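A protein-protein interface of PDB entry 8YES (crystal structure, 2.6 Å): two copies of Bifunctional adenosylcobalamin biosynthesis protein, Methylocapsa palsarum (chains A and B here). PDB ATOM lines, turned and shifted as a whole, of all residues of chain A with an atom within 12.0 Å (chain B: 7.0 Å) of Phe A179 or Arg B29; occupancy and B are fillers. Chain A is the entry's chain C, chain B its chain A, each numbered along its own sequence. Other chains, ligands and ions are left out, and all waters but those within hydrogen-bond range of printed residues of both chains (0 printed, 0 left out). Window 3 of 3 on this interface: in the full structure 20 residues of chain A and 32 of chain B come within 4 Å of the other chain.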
ATOM      1  N   PRO A 175     -27.100 -37.532 -14.167  1.00  0.00           N
ATOM      2  CA  PRO A 175     -26.805 -37.132 -15.535  1.00  0.00           C
ATOM      3  C   PRO A 175     -26.572 -35.629 -15.620  1.00  0.00           C
ATOM      4  O   PRO A 175     -27.118 -34.905 -14.856  1.00  0.00           O
ATOM      5  CB  PRO A 175     -28.056 -37.451 -16.349  1.00  0.00           C
ATOM      6  CG  PRO A 175     -28.897 -38.316 -15.434  1.00  0.00           C
ATOM      7  CD  PRO A 175     -28.485 -37.985 -14.013  1.00  0.00           C
ATOM      8  N   VAL A 176     -25.761 -35.213 -16.575  1.00  0.00           N
ATOM      9  CA  VAL A 176     -25.435 -33.780 -16.834  1.00  0.00           C
ATOM     10  C   VAL A 176     -25.375 -33.617 -18.357  1.00  0.00           C
ATOM     11  O   VAL A 176     -24.676 -34.402 -19.001  1.00  0.00           O
ATOM     12  CB  VAL A 176     -24.121 -33.412 -16.120  1.00  0.00           C
ATOM     13  CG1 VAL A 176     -22.910 -33.892 -16.911  1.00  0.00           C
ATOM     14  CG2 VAL A 176     -24.031 -31.933 -15.796  1.00  0.00           C
ATOM     15  N   PHE A 177     -26.160 -32.709 -18.918  1.00  0.00           N
ATOM     16  CA  PHE A 177     -26.434 -32.641 -20.378  1.00  0.00           C
ATOM     17  C   PHE A 177     -25.688 -31.465 -21.018  1.00  0.00           C
ATOM     18  O   PHE A 177     -25.310 -30.495 -20.352  1.00  0.00           O
ATOM     19  CB  PHE A 177     -27.945 -32.557 -20.607  1.00  0.00           C
ATOM     20  CG  PHE A 177     -28.644 -33.834 -20.241  1.00  0.00           C
ATOM     21  CD1 PHE A 177     -28.534 -34.955 -21.049  1.00  0.00           C
ATOM     22  CD2 PHE A 177     -29.354 -33.938 -19.056  1.00  0.00           C
ATOM     23  CE1 PHE A 177     -29.159 -36.142 -20.696  1.00  0.00           C
ATOM     24  CE2 PHE A 177     -29.968 -35.130 -18.703  1.00  0.00           C
ATOM     25  CZ  PHE A 177     -29.877 -36.223 -19.521  1.00  0.00           C
ATOM     26  N   ARG A 178     -25.532 -31.551 -22.330  1.00  0.00           N
ATOM     27  CA  ARG A 178     -24.677 -30.650 -23.134  1.00  0.00           C
ATOM     28  C   ARG A 178     -25.544 -30.048 -24.256  1.00  0.00           C
ATOM     29  O   ARG A 178     -25.857 -30.741 -25.248  1.00  0.00           O
ATOM     30  CB  ARG A 178     -23.479 -31.476 -23.602  1.00  0.00           C
ATOM     31  CG  ARG A 178     -22.349 -30.660 -24.190  1.00  0.00           C
ATOM     32  CD  ARG A 178     -21.383 -31.594 -24.874  1.00  0.00           C
ATOM     33  NE  ARG A 178     -20.230 -30.873 -25.387  1.00  0.00           N
ATOM     34  CZ  ARG A 178     -19.247 -31.417 -26.095  1.00  0.00           C
ATOM     35  NH1 ARG A 178     -19.260 -32.709 -26.388  1.00  0.00           N
ATOM     36  NH2 ARG A 178     -18.241 -30.660 -26.494  1.00  0.00           N
ATOM     37  N   PHE A 179     -25.981 -28.813 -24.063  1.00  0.00           N
ATOM     38  CA  PHE A 179     -26.897 -28.113 -24.983  1.00  0.00           C
ATOM     39  C   PHE A 179     -26.064 -27.398 -26.054  1.00  0.00           C
ATOM     40  O   PHE A 179     -24.835 -27.305 -25.911  1.00  0.00           O
ATOM     41  CB  PHE A 179     -27.804 -27.188 -24.176  1.00  0.00           C
ATOM     42  CG  PHE A 179     -28.775 -27.935 -23.307  1.00  0.00           C
ATOM     43  CD1 PHE A 179     -29.755 -28.723 -23.878  1.00  0.00           C
ATOM     44  CD2 PHE A 179     -28.664 -27.907 -21.931  1.00  0.00           C
ATOM     45  CE1 PHE A 179     -30.630 -29.455 -23.093  1.00  0.00           C
ATOM     46  CE2 PHE A 179     -29.554 -28.618 -21.146  1.00  0.00           C
ATOM     47  CZ  PHE A 179     -30.540 -29.384 -21.729  1.00  0.00           C
ATOM     48  N   ASP B   1     -21.893 -35.277 -25.503  1.00  0.00           N
ATOM     49  CA  ASP B   1     -22.780 -35.879 -26.552  1.00  0.00           C
ATOM     50  C   ASP B   1     -23.969 -34.942 -26.791  1.00  0.00           C
ATOM     51  O   ASP B   1     -24.994 -35.085 -26.143  1.00  0.00           O
ATOM     52  CB  ASP B   1     -23.191 -37.287 -26.110  1.00  0.00           C
ATOM     53  CG  ASP B   1     -23.180 -38.304 -27.231  1.00  0.00           C
ATOM     54  OD1 ASP B   1     -23.443 -37.896 -28.391  1.00  0.00           O
ATOM     55  OD2 ASP B   1     -22.894 -39.489 -26.930  1.00  0.00           O
ATOM     56  N   PRO B   2     -23.897 -33.962 -27.727  1.00  0.00           N
ATOM     57  CA  PRO B   2     -24.697 -32.736 -27.641  1.00  0.00           C
ATOM     58  C   PRO B   2     -26.177 -32.890 -28.015  1.00  0.00           C
ATOM     59  O   PRO B   2     -26.467 -33.619 -28.914  1.00  0.00           O
ATOM     60  CB  PRO B   2     -24.076 -31.778 -28.683  1.00  0.00           C
ATOM     61  CG  PRO B   2     -22.886 -32.508 -29.272  1.00  0.00           C
ATOM     62  CD  PRO B   2     -23.071 -33.979 -28.944  1.00  0.00           C
ATOM     63  N   ILE B   3     -27.063 -32.125 -27.379  1.00  0.00           N
ATOM     64  CA  ILE B   3     -28.538 -32.260 -27.542  1.00  0.00           C
ATOM     65  C   ILE B   3     -29.144 -30.869 -27.734  1.00  0.00           C
ATOM     66  O   ILE B   3     -28.450 -29.875 -27.431  1.00  0.00           O
ATOM     67  CB  ILE B   3     -29.166 -32.977 -26.321  1.00  0.00           C
ATOM     68  CG1 ILE B   3     -29.076 -32.122 -25.060  1.00  0.00           C
ATOM     69  CG2 ILE B   3     -28.562 -34.352 -26.087  1.00  0.00           C
ATOM     70  CD1 ILE B   3     -29.932 -32.633 -23.966  1.00  0.00           C
ATOM     71  N   LYS B   4     -30.404 -30.811 -28.176  1.00  0.00           N
ATOM     72  CA  LYS B   4     -31.142 -29.538 -28.361  1.00  0.00           C
ATOM     73  C   LYS B   4     -32.293 -29.447 -27.353  1.00  0.00           C
ATOM     74  O   LYS B   4     -32.724 -28.326 -27.046  1.00  0.00           O
ATOM     75  CB  LYS B   4     -31.634 -29.470 -29.810  1.00  0.00           C
ATOM     76  CG  LYS B   4     -31.687 -28.066 -30.398  1.00  0.00           C
ATOM     77  CD  LYS B   4     -30.842 -27.893 -31.644  1.00  0.00           C
ATOM     78  CE  LYS B   4     -30.128 -26.557 -31.669  1.00  0.00           C
ATOM     79  NZ  LYS B   4     -29.868 -26.100 -33.055  1.00  0.00           N
ATOM     80  N   SER B   5     -32.755 -30.592 -26.843  1.00  0.00           N
ATOM     81  CA  SER B   5     -34.066 -30.742 -26.165  1.00  0.00           C
ATOM     82  C   SER B   5     -33.989 -31.803 -25.061  1.00  0.00           C
ATOM     83  O   SER B   5     -33.531 -32.966 -25.310  1.00  0.00           O
ATOM     84  CB  SER B   5     -35.143 -31.093 -27.160  1.00  0.00           C
ATOM     85  OG  SER B   5     -34.823 -32.324 -27.791  1.00  0.00           O
ATOM     86  N   LEU B   6     -34.507 -31.424 -23.898  1.00  0.00           N
ATOM     87  CA  LEU B   6     -34.543 -32.252 -22.682  1.00  0.00           C
ATOM     88  C   LEU B   6     -35.957 -32.167 -22.111  1.00  0.00           C
ATOM     89  O   LEU B   6     -36.485 -31.036 -21.963  1.00  0.00           O
ATOM     90  CB  LEU B   6     -33.499 -31.724 -21.687  1.00  0.00           C
ATOM     91  CG  LEU B   6     -33.487 -32.427 -20.327  1.00  0.00           C
ATOM     92  CD1 LEU B   6     -33.352 -33.944 -20.513  1.00  0.00           C
ATOM     93  CD2 LEU B   6     -32.364 -31.900 -19.443  1.00  0.00           C
ATOM     94  N   ALA B  20     -33.856 -28.865 -13.628  1.00  0.00           N
ATOM     95  CA  ALA B  20     -33.900 -28.143 -14.913  1.00  0.00           C
ATOM     96  C   ALA B  20     -33.048 -26.882 -14.761  1.00  0.00           C
ATOM     97  O   ALA B  20     -32.290 -26.552 -15.701  1.00  0.00           O
ATOM     98  CB  ALA B  20     -35.326 -27.822 -15.301  1.00  0.00           C
ATOM     99  N   MET B  23     -29.123 -27.812 -14.950  1.00  0.00           N
ATOM    100  CA  MET B  23     -28.710 -28.109 -16.347  1.00  0.00           C
ATOM    101  C   MET B  23     -28.706 -26.812 -17.174  1.00  0.00           C
ATOM    102  O   MET B  23     -27.849 -26.684 -18.067  1.00  0.00           O
ATOM    103  CB  MET B  23     -29.652 -29.119 -17.013  1.00  0.00           C
ATOM    104  CG  MET B  23     -29.700 -30.485 -16.342  1.00  0.00           C
ATOM    105  SD  MET B  23     -28.082 -31.311 -16.217  1.00  0.00           S
ATOM    106  CE  MET B  23     -27.639 -30.841 -14.545  1.00  0.00           C
ATOM    107  N   ALA B  24     -29.619 -25.882 -16.881  1.00  0.00           N
ATOM    108  CA  ALA B  24     -29.756 -24.588 -17.585  1.00  0.00           C
ATOM    109  C   ALA B  24     -28.530 -23.721 -17.291  1.00  0.00           C
ATOM    110  O   ALA B  24     -27.898 -23.224 -18.236  1.00  0.00           O
ATOM    111  CB  ALA B  24     -31.045 -23.903 -17.168  1.00  0.00           C
ATOM    112  N   GLU B  25     -28.198 -23.570 -16.012  1.00  0.00           N
ATOM    113  CA  GLU B  25     -27.062 -22.745 -15.546  1.00  0.00           C
ATOM    114  C   GLU B  25     -25.726 -23.396 -15.954  1.00  0.00           C
ATOM    115  O   GLU B  25     -24.772 -22.645 -16.213  1.00  0.00           O
ATOM    116  CB  GLU B  25     -27.267 -22.479 -14.059  1.00  0.00           C
ATOM    117  CG  GLU B  25     -28.482 -21.588 -13.794  1.00  0.00           C
ATOM    118  CD  GLU B  25     -28.848 -21.374 -12.335  1.00  0.00           C
ATOM    119  OE1 GLU B  25     -29.620 -20.436 -12.035  1.00  0.00           O
ATOM    120  OE2 GLU B  25     -28.356 -22.135 -11.489  1.00  0.00           O
ATOM    121  N   ALA B  26     -25.685 -24.721 -16.126  1.00  0.00           N
ATOM    122  CA  ALA B  26     -24.494 -25.511 -16.538  1.00  0.00           C
ATOM    123  C   ALA B  26     -24.058 -25.198 -17.985  1.00  0.00           C
ATOM    124  O   ALA B  26     -22.904 -25.510 -18.333  1.00  0.00           O
ATOM    125  CB  ALA B  26     -24.797 -26.990 -16.415  1.00  0.00           C
ATOM    126  N   SER B  27     -24.956 -24.666 -18.810  1.00  0.00           N
ATOM    127  CA  SER B  27     -24.761 -24.476 -20.265  1.00  0.00           C
ATOM    128  C   SER B  27     -24.028 -23.148 -20.533  1.00  0.00           C
ATOM    129  O   SER B  27     -23.312 -23.052 -21.560  1.00  0.00           O
ATOM    130  CB  SER B  27     -26.080 -24.509 -20.985  1.00  0.00           C
ATOM    131  OG  SER B  27     -26.805 -23.315 -20.716  1.00  0.00           O
ATOM    132  N   GLY B  28     -24.224 -22.151 -19.674  1.00  0.00           N
ATOM    133  CA  GLY B  28     -23.611 -20.820 -19.837  1.00  0.00           C
ATOM    134  C   GLY B  28     -24.321 -19.949 -20.873  1.00  0.00           C
ATOM    135  O   GLY B  28     -23.940 -18.774 -21.008  1.00  0.00           O
ATOM    136  N   ARG B  29     -25.307 -20.473 -21.603  1.00  0.00           N
ATOM    137  CA  ARG B  29     -26.141 -19.643 -22.513  1.00  0.00           C
ATOM    138  C   ARG B  29     -26.897 -18.586 -21.707  1.00  0.00           C
ATOM    139  O   ARG B  29     -26.840 -18.630 -20.469  1.00  0.00           O
ATOM    140  CB  ARG B  29     -27.151 -20.497 -23.289  1.00  0.00           C
ATOM    141  CG  ARG B  29     -26.666 -20.954 -24.657  1.00  0.00           C
ATOM    142  CD  ARG B  29     -26.188 -22.375 -24.654  1.00  0.00           C
ATOM    143  NE  ARG B  29     -26.009 -22.899 -26.002  1.00  0.00           N
ATOM    144  CZ  ARG B  29     -25.445 -24.073 -26.287  1.00  0.00           C
ATOM    145  NH1 ARG B  29     -24.999 -24.855 -25.310  1.00  0.00           N
ATOM    146  NH2 ARG B  29     -25.335 -24.464 -27.547  1.00  0.00           N
ATOM    147  N   SER B  30     -27.600 -17.697 -22.405  1.00  0.00           N
ATOM    148  CA  SER B  30     -28.594 -16.738 -21.853  1.00  0.00           C
ATOM    149  C   SER B  30     -29.907 -17.488 -21.591  1.00  0.00           C
ATOM    150  O   SER B  30     -30.323 -18.290 -22.459  1.00  0.00           O
ATOM    151  CB  SER B  30     -28.813 -15.575 -22.792  1.00  0.00           C
ATOM    152  OG  SER B  30     -29.906 -14.765 -22.350  1.00  0.00           O
ATOM    153  N   LEU B  31     -30.534 -17.197 -20.452  1.00  0.00           N
ATOM    154  CA  LEU B  31     -31.519 -18.070 -19.773  1.00  0.00           C
ATOM    155  C   LEU B  31     -32.880 -17.363 -19.685  1.00  0.00           C
ATOM    156  O   LEU B  31     -32.976 -16.258 -19.091  1.00  0.00           O
ATOM    157  CB  LEU B  31     -30.984 -18.440 -18.381  1.00  0.00           C
ATOM    158  CG  LEU B  31     -29.595 -19.083 -18.350  1.00  0.00           C
ATOM    159  CD1 LEU B  31     -29.098 -19.218 -16.922  1.00  0.00           C
ATOM    160  CD2 LEU B  31     -29.581 -20.444 -19.034  1.00  0.00           C
ATOM    161  N   ARG B  58     -29.037 -13.602 -14.528  1.00  0.00           N
ATOM    162  CA  ARG B  58     -28.853 -14.368 -15.792  1.00  0.00           C
ATOM    163  C   ARG B  58     -30.205 -14.729 -16.445  1.00  0.00           C
ATOM    164  O   ARG B  58     -30.170 -15.203 -17.615  1.00  0.00           O
ATOM    165  CB  ARG B  58     -28.116 -15.678 -15.506  1.00  0.00           C
ATOM    166  CG  ARG B  58     -26.601 -15.578 -15.531  1.00  0.00           C
ATOM    167  CD  ARG B  58     -25.953 -16.902 -15.197  1.00  0.00           C
ATOM    168  NE  ARG B  58     -26.226 -17.263 -13.807  1.00  0.00           N
ATOM    169  CZ  ARG B  58     -25.979 -18.453 -13.259  1.00  0.00           C
ATOM    170  NH1 ARG B  58     -25.461 -19.439 -13.974  1.00  0.00           N
ATOM    171  NH2 ARG B  58     -26.264 -18.644 -11.987  1.00  0.00           N
ATOM    172  N   GLN B  77     -33.308 -19.550 -30.030  1.00  0.00           N
ATOM    173  CA  GLN B  77     -32.125 -19.248 -30.884  1.00  0.00           C
ATOM    174  C   GLN B  77     -30.844 -19.696 -30.188  1.00  0.00           C
ATOM    175  O   GLN B  77     -30.841 -19.873 -28.977  1.00  0.00           O
ATOM    176  CB  GLN B  77     -32.099 -17.756 -31.234  1.00  0.00           C
ATOM    177  CG  GLN B  77     -32.342 -16.827 -30.055  1.00  0.00           C
ATOM    178  CD  GLN B  77     -32.359 -15.357 -30.409  1.00  0.00           C
ATOM    179  OE1 GLN B  77     -32.805 -14.518 -29.625  1.00  0.00           O
ATOM    180  NE2 GLN B  77     -31.849 -15.011 -31.583  1.00  0.00           N
ATOM    181  N   PRO B  78     -29.719 -19.882 -30.920  1.00  0.00           N
ATOM    182  CA  PRO B  78     -28.543 -20.598 -30.402  1.00  0.00           C
ATOM    183  C   PRO B  78     -27.818 -19.972 -29.203  1.00  0.00           C
ATOM    184  O   PRO B  78     -27.082 -20.671 -28.548  1.00  0.00           O
ATOM    185  CB  PRO B  78     -27.556 -20.595 -31.576  1.00  0.00           C
ATOM    186  CG  PRO B  78     -28.436 -20.383 -32.788  1.00  0.00           C
ATOM    187  CD  PRO B  78     -29.526 -19.450 -32.308  1.00  0.00           C
ATOM    188  N   GLU B  79     -28.044 -18.682 -28.953  1.00  0.00           N
ATOM    189  CA  GLU B  79     -27.479 -17.928 -27.797  1.00  0.00           C
ATOM    190  C   GLU B  79     -28.308 -18.210 -26.541  1.00  0.00           C
ATOM    191  O   GLU B  79     -27.978 -17.664 -25.473  1.00  0.00           O
ATOM    192  CB  GLU B  79     -27.510 -16.404 -28.017  1.00  0.00           C
ATOM    193  CG  GLU B  79     -27.125 -15.933 -29.414  1.00  0.00           C
ATOM    194  CD  GLU B  79     -28.300 -15.765 -30.359  1.00  0.00           C
ATOM    195  OE1 GLU B  79     -28.225 -16.272 -31.503  1.00  0.00           O
ATOM    196  OE2 GLU B  79     -29.294 -15.140 -29.937  1.00  0.00           O
ATOM    197  N   ARG B  80     -29.399 -18.956 -26.662  1.00  0.00           N
ATOM    198  CA  ARG B  80     -30.452 -18.981 -25.618  1.00  0.00           C
ATOM    199  C   ARG B  80     -30.727 -20.420 -25.203  1.00  0.00           C
ATOM    200  O   ARG B  80     -30.540 -21.317 -26.035  1.00  0.00           O
ATOM    201  CB  ARG B  80     -31.706 -18.292 -26.135  1.00  0.00           C
ATOM    202  CG  ARG B  80     -31.620 -16.778 -26.064  1.00  0.00           C
ATOM    203  CD  ARG B  80     -32.885 -16.147 -26.586  1.00  0.00           C
ATOM    204  NE  ARG B  80     -33.157 -14.901 -25.903  1.00  0.00           N
ATOM    205  CZ  ARG B  80     -34.345 -14.312 -25.861  1.00  0.00           C
ATOM    206  NH1 ARG B  80     -35.391 -14.864 -26.466  1.00  0.00           N
ATOM    207  NH2 ARG B  80     -34.474 -13.183 -25.181  1.00  0.00           N
ATOM    208  N   LEU B  81     -31.068 -20.615 -23.934  1.00  0.00           N
ATOM    209  CA  LEU B  81     -31.736 -21.847 -23.453  1.00  0.00           C
ATOM    210  C   LEU B  81     -33.070 -21.439 -22.855  1.00  0.00           C
ATOM    211  O   LEU B  81     -33.080 -20.524 -21.981  1.00  0.00           O
ATOM    212  CB  LEU B  81     -30.875 -22.535 -22.405  1.00  0.00           C
ATOM    213  CG  LEU B  81     -31.208 -24.002 -22.193  1.00  0.00           C
ATOM    214  CD1 LEU B  81     -29.947 -24.850 -22.223  1.00  0.00           C
ATOM    215  CD2 LEU B  81     -31.960 -24.171 -20.895  1.00  0.00           C
ATOM    216  N   PRO B 118     -31.773 -24.554 -28.094  1.00  0.00           N
ATOM    217  CA  PRO B 118     -32.111 -25.564 -27.087  1.00  0.00           C
ATOM    218  C   PRO B 118     -33.238 -25.262 -26.092  1.00  0.00           C
ATOM    219  O   PRO B 118     -33.411 -24.127 -25.679  1.00  0.00           O
ATOM    220  CB  PRO B 118     -30.827 -25.678 -26.249  1.00  0.00           C
ATOM    221  CG  PRO B 118     -30.198 -24.322 -26.381  1.00  0.00           C
ATOM    222  CD  PRO B 118     -30.457 -23.953 -27.830  1.00  0.00           C
ATOM    223  N   VAL B 119     -33.941 -26.306 -25.658  1.00  0.00           N
ATOM    224  CA  VAL B 119     -35.120 -26.141 -24.752  1.00  0.00           C
ATOM    225  C   VAL B 119     -35.187 -27.305 -23.756  1.00  0.00           C
ATOM    226  O   VAL B 119     -34.903 -28.462 -24.147  1.00  0.00           O
ATOM    227  CB  VAL B 119     -36.417 -25.998 -25.563  1.00  0.00           C
ATOM    228  CG1 VAL B 119     -36.656 -27.224 -26.416  1.00  0.00           C
ATOM    229  CG2 VAL B 119     -37.612 -25.736 -24.677  1.00  0.00           C
ATOM    230  N   ILE B 120     -35.514 -26.973 -22.501  1.00  0.00           N
ATOM    231  CA  ILE B 120     -35.827 -27.946 -21.418  1.00  0.00           C
ATOM    232  C   ILE B 120     -37.320 -27.848 -21.131  1.00  0.00           C
ATOM    233  O   ILE B 120     -37.782 -26.749 -20.749  1.00  0.00           O
ATOM    234  CB  ILE B 120     -34.971 -27.673 -20.166  1.00  0.00           C
ATOM    235  CG1 ILE B 120     -33.482 -27.713 -20.530  1.00  0.00           C
ATOM    236  CG2 ILE B 120     -35.308 -28.652 -19.038  1.00  0.00           C
ATOM    237  CD1 ILE B 120     -32.553 -27.326 -19.406  1.00  0.00           C
ATOM    238  N   ALA B 157     -33.069 -36.141 -25.177  1.00  0.00           N
ATOM    239  CA  ALA B 157     -32.828 -36.742 -23.853  1.00  0.00           C
ATOM    240  C   ALA B 157     -34.105 -36.665 -23.016  1.00  0.00           C
ATOM    241  O   ALA B 157     -34.840 -35.682 -23.146  1.00  0.00           O
ATOM    242  CB  ALA B 157     -31.681 -36.037 -23.173  1.00  0.00           C
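N of Leu B6 is in hydrogen-bond range of O of Val B119 (3.0 Å).
The side-chain hydroxyl of Ser B27 lies close to the backbone NH of Arg B29 (3.3 Å).
The backbone carbonyl oxygen (O) of Ser B30 lies within hydrogen-bond range of the backbone NH (N) of Leu B81 (2.9 Å).
N of Ala B157 is in hydrogen-bond range of O of Ser B5, 3.2 Å away.
Of the printed residues of chain B, Phe A179 touches Ile B3, Leu B6, Arg B29, Leu B81, Pro B118 and Ile B120.
Arg B29 touches just one residue of chain A: Phe A179 (2.5 Å).
Pro B2 touches just one residue of chain A: Arg A178.
No residue of chain A comes within 4 Å of Ala B24.
No residue of chain A comes within 4 Å of Ala B26.
No residue of chain A comes within 4 Å of Ser B27.
No residue of chain A comes within 4 Å of Ser B30.
No residue of chain A comes within 4 Å of Leu B31.
Of chain A, only Phe A179 comes within 4 Å of Leu B81.
Printed residues of chain B within 4 Å of Val A176: Met B23.
Of the printed residues of chain A, Met B23 touches Pro A175, Val A176 and Phe A177.
Of the printed residues of chain B, Arg A178 touches Asp B1, Pro B2 and Ile B3.
Of the printed residues of chain B, Phe A177 touches Ile B3, Leu B6, Met B23 and Ala B157.
Printed residues of chain A within 4 Å of Ala B157: Phe A177 (3.5 Å).
Arg B58 touches none of the printed residues of chain A.
The nearest printed residue of chain B that does not touch Phe A179 is Met B23 (4.02 Å).
The nearest printed residue of chain A that does not touch Met B23 is Phe A179 (4.02 Å).
Hydrophobic or aromatic side chains of chain B that line the printed part of chain A: Ile B3, Leu B6, Met B23, Leu B81, Pro B118, Ile B120 and Ala B157.
Hydrophobic or aromatic side chains of chain A within 4 Å of the printed part of chain B: Val A176, Phe A177 and Phe A179.
Among the printed residues, no Asp or Glu carboxylate lies within 4 Å of a Lys or Arg side-chain nitrogen of the other chain.
No position is printed for both chains.
Of the 15 pairs that touch across the chains among the printed residues, none has its exchanged pair printed and touching as well.
Among the printed residues, merely in contact across the chains: Pro A175 with Met B23, Val A176 with Met B23, Phe A177 with Ile B3, Phe A177 with Leu B6, Phe A177 with Ala B157, Arg A178 with Asp B1, Arg A178 with Pro B2, Phe A179 with Ile B3, Phe A179 with Leu B6, Phe A179 with Leu B81, Phe A179 with Pro B118 and Phe A179 with Ile B120.
SD of Met B23 is in hydrogen-bond range of N of Phe A177 (3.6 Å).
NH1 of Arg B29 is in hydrogen-bond range of O of Phe A179 (2.5 Å).
The backbone carbonyl oxygen (O) of Arg A178 sits at hydrogen-bond distance from the backbone NH (N) of Ile B3, at 2.8 Å.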
